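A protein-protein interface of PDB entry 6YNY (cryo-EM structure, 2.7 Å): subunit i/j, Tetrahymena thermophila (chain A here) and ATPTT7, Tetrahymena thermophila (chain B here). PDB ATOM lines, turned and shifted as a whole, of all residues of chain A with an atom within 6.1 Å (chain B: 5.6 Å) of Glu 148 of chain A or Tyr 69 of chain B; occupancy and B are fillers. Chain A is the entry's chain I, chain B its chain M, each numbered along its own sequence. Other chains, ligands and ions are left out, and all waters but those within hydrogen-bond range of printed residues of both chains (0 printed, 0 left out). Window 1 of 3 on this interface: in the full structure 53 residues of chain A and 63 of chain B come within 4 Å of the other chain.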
ATOM      1  N   TYR A 116     -27.940 -22.408   5.342  1.00  0.00           N
ATOM      2  CA  TYR A 116     -28.556 -22.748   4.064  1.00  0.00           C
ATOM      3  C   TYR A 116     -27.828 -23.970   3.522  1.00  0.00           C
ATOM      4  O   TYR A 116     -26.746 -23.859   2.943  1.00  0.00           O
ATOM      5  CB  TYR A 116     -28.485 -21.561   3.115  1.00  0.00           C
ATOM      6  CG  TYR A 116     -29.133 -21.780   1.777  1.00  0.00           C
ATOM      7  CD1 TYR A 116     -30.499 -21.959   1.668  1.00  0.00           C
ATOM      8  CD2 TYR A 116     -28.380 -21.783   0.619  1.00  0.00           C
ATOM      9  CE1 TYR A 116     -31.092 -22.153   0.444  1.00  0.00           C
ATOM     10  CE2 TYR A 116     -28.962 -21.973  -0.604  1.00  0.00           C
ATOM     11  CZ  TYR A 116     -30.316 -22.156  -0.690  1.00  0.00           C
ATOM     12  OH  TYR A 116     -30.886 -22.346  -1.921  1.00  0.00           O
ATOM     13  N   PRO A 118     -28.091 -26.051   0.968  1.00  0.00           N
ATOM     14  CA  PRO A 118     -27.664 -26.225  -0.429  1.00  0.00           C
ATOM     15  C   PRO A 118     -26.317 -25.607  -0.747  1.00  0.00           C
ATOM     16  O   PRO A 118     -25.728 -25.951  -1.778  1.00  0.00           O
ATOM     17  CB  PRO A 118     -28.793 -25.559  -1.222  1.00  0.00           C
ATOM     18  CG  PRO A 118     -29.953 -25.614  -0.329  1.00  0.00           C
ATOM     19  CD  PRO A 118     -29.418 -25.426   1.043  1.00  0.00           C
ATOM     20  N   THR A 142     -21.322 -26.300 -13.732  1.00  0.00           N
ATOM     21  CA  THR A 142     -21.711 -25.585 -14.934  1.00  0.00           C
ATOM     22  C   THR A 142     -22.781 -24.562 -14.587  1.00  0.00           C
ATOM     23  O   THR A 142     -23.656 -24.817 -13.757  1.00  0.00           O
ATOM     24  CB  THR A 142     -22.229 -26.556 -15.995  1.00  0.00           C
ATOM     25  OG1 THR A 142     -21.200 -27.490 -16.337  1.00  0.00           O
ATOM     26  CG2 THR A 142     -22.673 -25.815 -17.239  1.00  0.00           C
ATOM     27  N   SER A 143     -22.706 -23.403 -15.230  1.00  0.00           N
ATOM     28  CA  SER A 143     -23.595 -22.298 -14.900  1.00  0.00           C
ATOM     29  C   SER A 143     -25.056 -22.709 -14.993  1.00  0.00           C
ATOM     30  O   SER A 143     -25.494 -23.280 -15.995  1.00  0.00           O
ATOM     31  CB  SER A 143     -23.328 -21.120 -15.831  1.00  0.00           C
ATOM     32  OG  SER A 143     -24.181 -20.032 -15.532  1.00  0.00           O
ATOM     33  N   ALA A 144     -25.811 -22.415 -13.935  1.00  0.00           N
ATOM     34  CA  ALA A 144     -27.248 -22.634 -13.964  1.00  0.00           C
ATOM     35  C   ALA A 144     -27.939 -21.699 -14.942  1.00  0.00           C
ATOM     36  O   ALA A 144     -29.027 -22.022 -15.429  1.00  0.00           O
ATOM     37  CB  ALA A 144     -27.834 -22.452 -12.568  1.00  0.00           C
ATOM     38  N   HIS A 145     -27.337 -20.546 -15.230  1.00  0.00           N
ATOM     39  CA  HIS A 145     -27.895 -19.645 -16.229  1.00  0.00           C
ATOM     40  C   HIS A 145     -27.925 -20.311 -17.597  1.00  0.00           C
ATOM     41  O   HIS A 145     -28.940 -20.277 -18.299  1.00  0.00           O
ATOM     42  CB  HIS A 145     -27.078 -18.358 -16.285  1.00  0.00           C
ATOM     43  CG  HIS A 145     -27.212 -17.494 -15.072  1.00  0.00           C
ATOM     44  ND1 HIS A 145     -26.300 -16.509 -14.763  1.00  0.00           N
ATOM     45  CD2 HIS A 145     -28.152 -17.455 -14.099  1.00  0.00           C
ATOM     46  CE1 HIS A 145     -26.668 -15.907 -13.648  1.00  0.00           C
ATOM     47  NE2 HIS A 145     -27.789 -16.461 -13.225  1.00  0.00           N
ATOM     48  N   TYR A 146     -26.808 -20.922 -17.991  1.00  0.00           N
ATOM     49  CA  TYR A 146     -26.738 -21.585 -19.286  1.00  0.00           C
ATOM     50  C   TYR A 146     -27.749 -22.715 -19.383  1.00  0.00           C
ATOM     51  O   TYR A 146     -28.429 -22.865 -20.403  1.00  0.00           O
ATOM     52  CB  TYR A 146     -25.326 -22.112 -19.526  1.00  0.00           C
ATOM     53  CG  TYR A 146     -25.211 -23.012 -20.728  1.00  0.00           C
ATOM     54  CD1 TYR A 146     -25.084 -22.489 -22.001  1.00  0.00           C
ATOM     55  CD2 TYR A 146     -25.229 -24.386 -20.588  1.00  0.00           C
ATOM     56  CE1 TYR A 146     -24.984 -23.306 -23.094  1.00  0.00           C
ATOM     57  CE2 TYR A 146     -25.130 -25.210 -21.677  1.00  0.00           C
ATOM     58  CZ  TYR A 146     -25.006 -24.667 -22.930  1.00  0.00           C
ATOM     59  OH  TYR A 146     -24.905 -25.486 -24.026  1.00  0.00           O
ATOM     60  N   ILE A 147     -27.866 -23.520 -18.328  1.00  0.00           N
ATOM     61  CA  ILE A 147     -28.733 -24.690 -18.377  1.00  0.00           C
ATOM     62  C   ILE A 147     -30.180 -24.280 -18.609  1.00  0.00           C
ATOM     63  O   ILE A 147     -30.906 -24.922 -19.376  1.00  0.00           O
ATOM     64  CB  ILE A 147     -28.572 -25.513 -17.090  1.00  0.00           C
ATOM     65  CG1 ILE A 147     -27.137 -26.019 -16.983  1.00  0.00           C
ATOM     66  CG2 ILE A 147     -29.552 -26.658 -17.069  1.00  0.00           C
ATOM     67  CD1 ILE A 147     -26.801 -26.650 -15.677  1.00  0.00           C
ATOM     68  N   GLU A 148     -30.622 -23.210 -17.957  1.00  0.00           N
ATOM     69  CA  GLU A 148     -32.010 -22.786 -18.067  1.00  0.00           C
ATOM     70  C   GLU A 148     -32.234 -21.854 -19.247  1.00  0.00           C
ATOM     71  O   GLU A 148     -33.280 -21.925 -19.901  1.00  0.00           O
ATOM     72  CB  GLU A 148     -32.455 -22.108 -16.776  1.00  0.00           C
ATOM     73  CG  GLU A 148     -32.469 -23.028 -15.578  1.00  0.00           C
ATOM     74  CD  GLU A 148     -33.470 -24.157 -15.713  1.00  0.00           C
ATOM     75  OE1 GLU A 148     -34.332 -24.091 -16.614  1.00  0.00           O
ATOM     76  OE2 GLU A 148     -33.394 -25.115 -14.917  1.00  0.00           O
ATOM     77  N   ILE A 149     -31.275 -20.973 -19.532  1.00  0.00           N
ATOM     78  CA  ILE A 149     -31.419 -20.069 -20.665  1.00  0.00           C
ATOM     79  C   ILE A 149     -31.290 -20.836 -21.973  1.00  0.00           C
ATOM     80  O   ILE A 149     -31.996 -20.552 -22.947  1.00  0.00           O
ATOM     81  CB  ILE A 149     -30.392 -18.928 -20.565  1.00  0.00           C
ATOM     82  CG1 ILE A 149     -30.704 -18.065 -19.344  1.00  0.00           C
ATOM     83  CG2 ILE A 149     -30.397 -18.095 -21.831  1.00  0.00           C
ATOM     84  CD1 ILE A 149     -29.685 -17.005 -19.054  1.00  0.00           C
ATOM     85  N   ASN A 150     -30.389 -21.817 -22.019  1.00  0.00           N
ATOM     86  CA  ASN A 150     -30.245 -22.633 -23.218  1.00  0.00           C
ATOM     87  C   ASN A 150     -31.448 -23.540 -23.422  1.00  0.00           C
ATOM     88  O   ASN A 150     -31.804 -23.850 -24.563  1.00  0.00           O
ATOM     89  CB  ASN A 150     -28.962 -23.457 -23.137  1.00  0.00           C
ATOM     90  CG  ASN A 150     -28.729 -24.297 -24.365  1.00  0.00           C
ATOM     91  OD1 ASN A 150     -28.419 -23.780 -25.435  1.00  0.00           O
ATOM     92  ND2 ASN A 150     -28.861 -25.605 -24.214  1.00  0.00           N
ATOM     93  N   ALA A 151     -32.084 -23.972 -22.334  1.00  0.00           N
ATOM     94  CA  ALA A 151     -33.272 -24.806 -22.453  1.00  0.00           C
ATOM     95  C   ALA A 151     -34.423 -24.032 -23.080  1.00  0.00           C
ATOM     96  O   ALA A 151     -35.219 -24.596 -23.839  1.00  0.00           O
ATOM     97  CB  ALA A 151     -33.667 -25.338 -21.081  1.00  0.00           C
ATOM     98  N   ILE A 152     -34.533 -22.743 -22.765  1.00  0.00           N
ATOM     99  CA  ILE A 152     -35.550 -21.904 -23.381  1.00  0.00           C
ATOM    100  C   ILE A 152     -35.129 -21.501 -24.787  1.00  0.00           C
ATOM    101  O   ILE A 152     -35.956 -21.441 -25.702  1.00  0.00           O
ATOM    102  CB  ILE A 152     -35.814 -20.673 -22.498  1.00  0.00           C
ATOM    103  CG1 ILE A 152     -36.335 -21.102 -21.130  1.00  0.00           C
ATOM    104  CG2 ILE A 152     -36.794 -19.742 -23.171  1.00  0.00           C
ATOM    105  CD1 ILE A 152     -36.354 -19.996 -20.112  1.00  0.00           C
ATOM    106  N   TYR A 153     -33.841 -21.219 -24.974  1.00  0.00           N
ATOM    107  CA  TYR A 153     -33.344 -20.792 -26.275  1.00  0.00           C
ATOM    108  C   TYR A 153     -33.581 -21.860 -27.334  1.00  0.00           C
ATOM    109  O   TYR A 153     -34.038 -21.563 -28.442  1.00  0.00           O
ATOM    110  CB  TYR A 153     -31.859 -20.456 -26.159  1.00  0.00           C
ATOM    111  CG  TYR A 153     -31.179 -20.109 -27.456  1.00  0.00           C
ATOM    112  CD1 TYR A 153     -31.250 -18.832 -27.979  1.00  0.00           C
ATOM    113  CD2 TYR A 153     -30.445 -21.055 -28.147  1.00  0.00           C
ATOM    114  CE1 TYR A 153     -30.623 -18.513 -29.157  1.00  0.00           C
ATOM    115  CE2 TYR A 153     -29.817 -20.747 -29.322  1.00  0.00           C
ATOM    116  CZ  TYR A 153     -29.906 -19.476 -29.826  1.00  0.00           C
ATOM    117  OH  TYR A 153     -29.271 -19.177 -31.005  1.00  0.00           O
ATOM    118  N   MET B  67     -22.951 -20.020 -11.831  1.00  0.00           N
ATOM    119  CA  MET B  67     -24.020 -19.706 -10.903  1.00  0.00           C
ATOM    120  C   MET B  67     -24.713 -20.970 -10.411  1.00  0.00           C
ATOM    121  O   MET B  67     -24.776 -21.986 -11.107  1.00  0.00           O
ATOM    122  CB  MET B  67     -25.034 -18.782 -11.567  1.00  0.00           C
ATOM    123  CG  MET B  67     -26.101 -18.283 -10.640  1.00  0.00           C
ATOM    124  SD  MET B  67     -25.419 -17.415  -9.228  1.00  0.00           S
ATOM    125  CE  MET B  67     -26.910 -17.136  -8.307  1.00  0.00           C
ATOM    126  N   THR B  68     -25.232 -20.894  -9.194  1.00  0.00           N
ATOM    127  CA  THR B  68     -25.939 -21.995  -8.563  1.00  0.00           C
ATOM    128  C   THR B  68     -27.444 -21.804  -8.690  1.00  0.00           C
ATOM    129  O   THR B  68     -27.937 -20.747  -9.087  1.00  0.00           O
ATOM    130  CB  THR B  68     -25.550 -22.108  -7.088  1.00  0.00           C
ATOM    131  OG1 THR B  68     -25.886 -20.896  -6.406  1.00  0.00           O
ATOM    132  CG2 THR B  68     -24.080 -22.355  -6.950  1.00  0.00           C
ATOM    133  N   TYR B  69     -28.177 -22.854  -8.333  1.00  0.00           N
ATOM    134  CA  TYR B  69     -29.630 -22.810  -8.328  1.00  0.00           C
ATOM    135  C   TYR B  69     -30.106 -22.368  -6.953  1.00  0.00           C
ATOM    136  O   TYR B  69     -29.922 -23.114  -5.980  1.00  0.00           O
ATOM    137  CB  TYR B  69     -30.213 -24.169  -8.671  1.00  0.00           C
ATOM    138  CG  TYR B  69     -30.211 -24.508 -10.139  1.00  0.00           C
ATOM    139  CD1 TYR B  69     -31.192 -24.017 -10.979  1.00  0.00           C
ATOM    140  CD2 TYR B  69     -29.244 -25.335 -10.681  1.00  0.00           C
ATOM    141  CE1 TYR B  69     -31.204 -24.328 -12.313  1.00  0.00           C
ATOM    142  CE2 TYR B  69     -29.250 -25.651 -12.016  1.00  0.00           C
ATOM    143  CZ  TYR B  69     -30.231 -25.144 -12.828  1.00  0.00           C
ATOM    144  OH  TYR B  69     -30.242 -25.458 -14.163  1.00  0.00           O
ATOM    145  N   PRO B  70     -30.705 -21.186  -6.811  1.00  0.00           N
ATOM    146  CA  PRO B  70     -31.281 -20.812  -5.516  1.00  0.00           C
ATOM    147  C   PRO B  70     -32.560 -21.590  -5.251  1.00  0.00           C
ATOM    148  O   PRO B  70     -33.429 -21.700  -6.117  1.00  0.00           O
ATOM    149  CB  PRO B  70     -31.547 -19.312  -5.671  1.00  0.00           C
ATOM    150  CG  PRO B  70     -31.717 -19.118  -7.106  1.00  0.00           C
ATOM    151  CD  PRO B  70     -30.823 -20.094  -7.787  1.00  0.00           C
ATOM    152  N   THR B  71     -32.667 -22.138  -4.044  1.00  0.00           N
ATOM    153  CA  THR B  71     -33.797 -22.965  -3.663  1.00  0.00           C
ATOM    154  C   THR B  71     -34.427 -22.418  -2.394  1.00  0.00           C
ATOM    155  O   THR B  71     -33.894 -21.519  -1.740  1.00  0.00           O
ATOM    156  CB  THR B  71     -33.389 -24.426  -3.432  1.00  0.00           C
ATOM    157  OG1 THR B  71     -32.783 -24.556  -2.141  1.00  0.00           O
ATOM    158  CG2 THR B  71     -32.405 -24.877  -4.471  1.00  0.00           C
ATOM    159  N   PHE B 136     -33.965 -14.972  -9.980  1.00  0.00           N
ATOM    160  CA  PHE B 136     -33.350 -15.921 -10.894  1.00  0.00           C
ATOM    161  C   PHE B 136     -34.305 -16.302 -12.014  1.00  0.00           C
ATOM    162  O   PHE B 136     -33.906 -16.373 -13.181  1.00  0.00           O
ATOM    163  CB  PHE B 136     -32.910 -17.153 -10.111  1.00  0.00           C
ATOM    164  CG  PHE B 136     -32.271 -18.214 -10.946  1.00  0.00           C
ATOM    165  CD1 PHE B 136     -30.922 -18.169 -11.223  1.00  0.00           C
ATOM    166  CD2 PHE B 136     -33.014 -19.266 -11.437  1.00  0.00           C
ATOM    167  CE1 PHE B 136     -30.334 -19.148 -11.983  1.00  0.00           C
ATOM    168  CE2 PHE B 136     -32.429 -20.241 -12.193  1.00  0.00           C
ATOM    169  CZ  PHE B 136     -31.088 -20.185 -12.467  1.00  0.00           C
ATOM    170  N   ILE B 140     -33.461 -15.426 -16.243  1.00  0.00           N
ATOM    171  CA  ILE B 140     -33.262 -16.439 -17.272  1.00  0.00           C
ATOM    172  C   ILE B 140     -34.272 -16.275 -18.394  1.00  0.00           C
ATOM    173  O   ILE B 140     -33.993 -16.620 -19.548  1.00  0.00           O
ATOM    174  CB  ILE B 140     -33.338 -17.841 -16.646  1.00  0.00           C
ATOM    175  CG1 ILE B 140     -34.704 -18.061 -16.007  1.00  0.00           C
ATOM    176  CG2 ILE B 140     -32.247 -18.007 -15.610  1.00  0.00           C
ATOM    177  CD1 ILE B 140     -34.919 -19.450 -15.526  1.00  0.00           C
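Among the printed residues, merely in contact across the chains: Tyr 116 of chain A with Pro 70 of chain B (3.8 Å), Pro 118 of chain A with Thr 71 of chain B (3.5 Å), Ser 143 of chain A with Met 67 of chain B (3.9 Å), Ala 144 of chain A with Thr 68 of chain B (3.9 Å), Ala 144 of chain A with Tyr 69 of chain B (3.5 Å), Ala 144 of chain A with Phe 136 of chain B (3.97 Å), His 145 of chain A with Met 67 of chain B (3.6 Å), His 145 of chain A with Phe 136 of chain B (3.5 Å), Ile 147 of chain A with Tyr 69 of chain B (3.2 Å), Glu 148 of chain A with Ile 140 of chain B (3.8 Å) and Ile 149 of chain A with Ile 140 of chain B (3.6 Å).
Of chain B, only Tyr 69 and Ile 140 come within 4 Å of Glu 148 of chain A.
Of chain A, only Ala 144, Ile 147 and Glu 148 come within 4 Å of Tyr 69 of chain B.
Of the printed residues of chain A, Met 67 of chain B touches Ser 143, Ala 144 and His 145.
Of the printed residues of chain B, Ser 143 of chain A touches Met 67 (3.9 Å).
Ala 151 of chain A touches none of the printed residues of chain B.
Asn 150 of chain A touches none of the printed residues of chain B.
The nearest residue of chain A that does not touch Tyr 69 of chain B is Tyr 116 of chain A (4.2 Å).
The side-chain hydroxyl (OG) of Ser 143 of chain A sits close to the backbone NH (N) of His 145 of chain A (3.2 Å).
Printed residues of chain B that touch a printed residue of chain A: Met 67, Thr 68, Tyr 69, Pro 70, Thr 71, Phe 136 and Ile 140.
Hydrophobic or aromatic side chains of chain B within 4 Å of the printed part of chain A: Met 67, Tyr 69, Phe 136 and Ile 140.
Of the 14 printed residues of chain A, 8 touch a printed residue of chain B.
Printed residues of chain A that touch a printed residue of chain B: Tyr 116, Pro 118, Ser 143, Ala 144, His 145, Ile 147, Glu 148 and Ile 149.
Among the printed residues, no Asp or Glu carboxylate lies within 4 Å of a Lys or Arg side-chain nitrogen of the other chain.
The side-chain carboxylate of Glu 148 of chain A lies within hydrogen-bond range of the side-chain hydroxyl of Tyr 69 of chain B.
The side-chain hydroxyl (OH) of Tyr 116 of chain A is in hydrogen-bond range of the backbone NH (N) of Thr 71 of chain B (2.8 Å).
O of Met 67 of chain B lies within hydrogen-bond range of N of Ala 144 of chain A.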
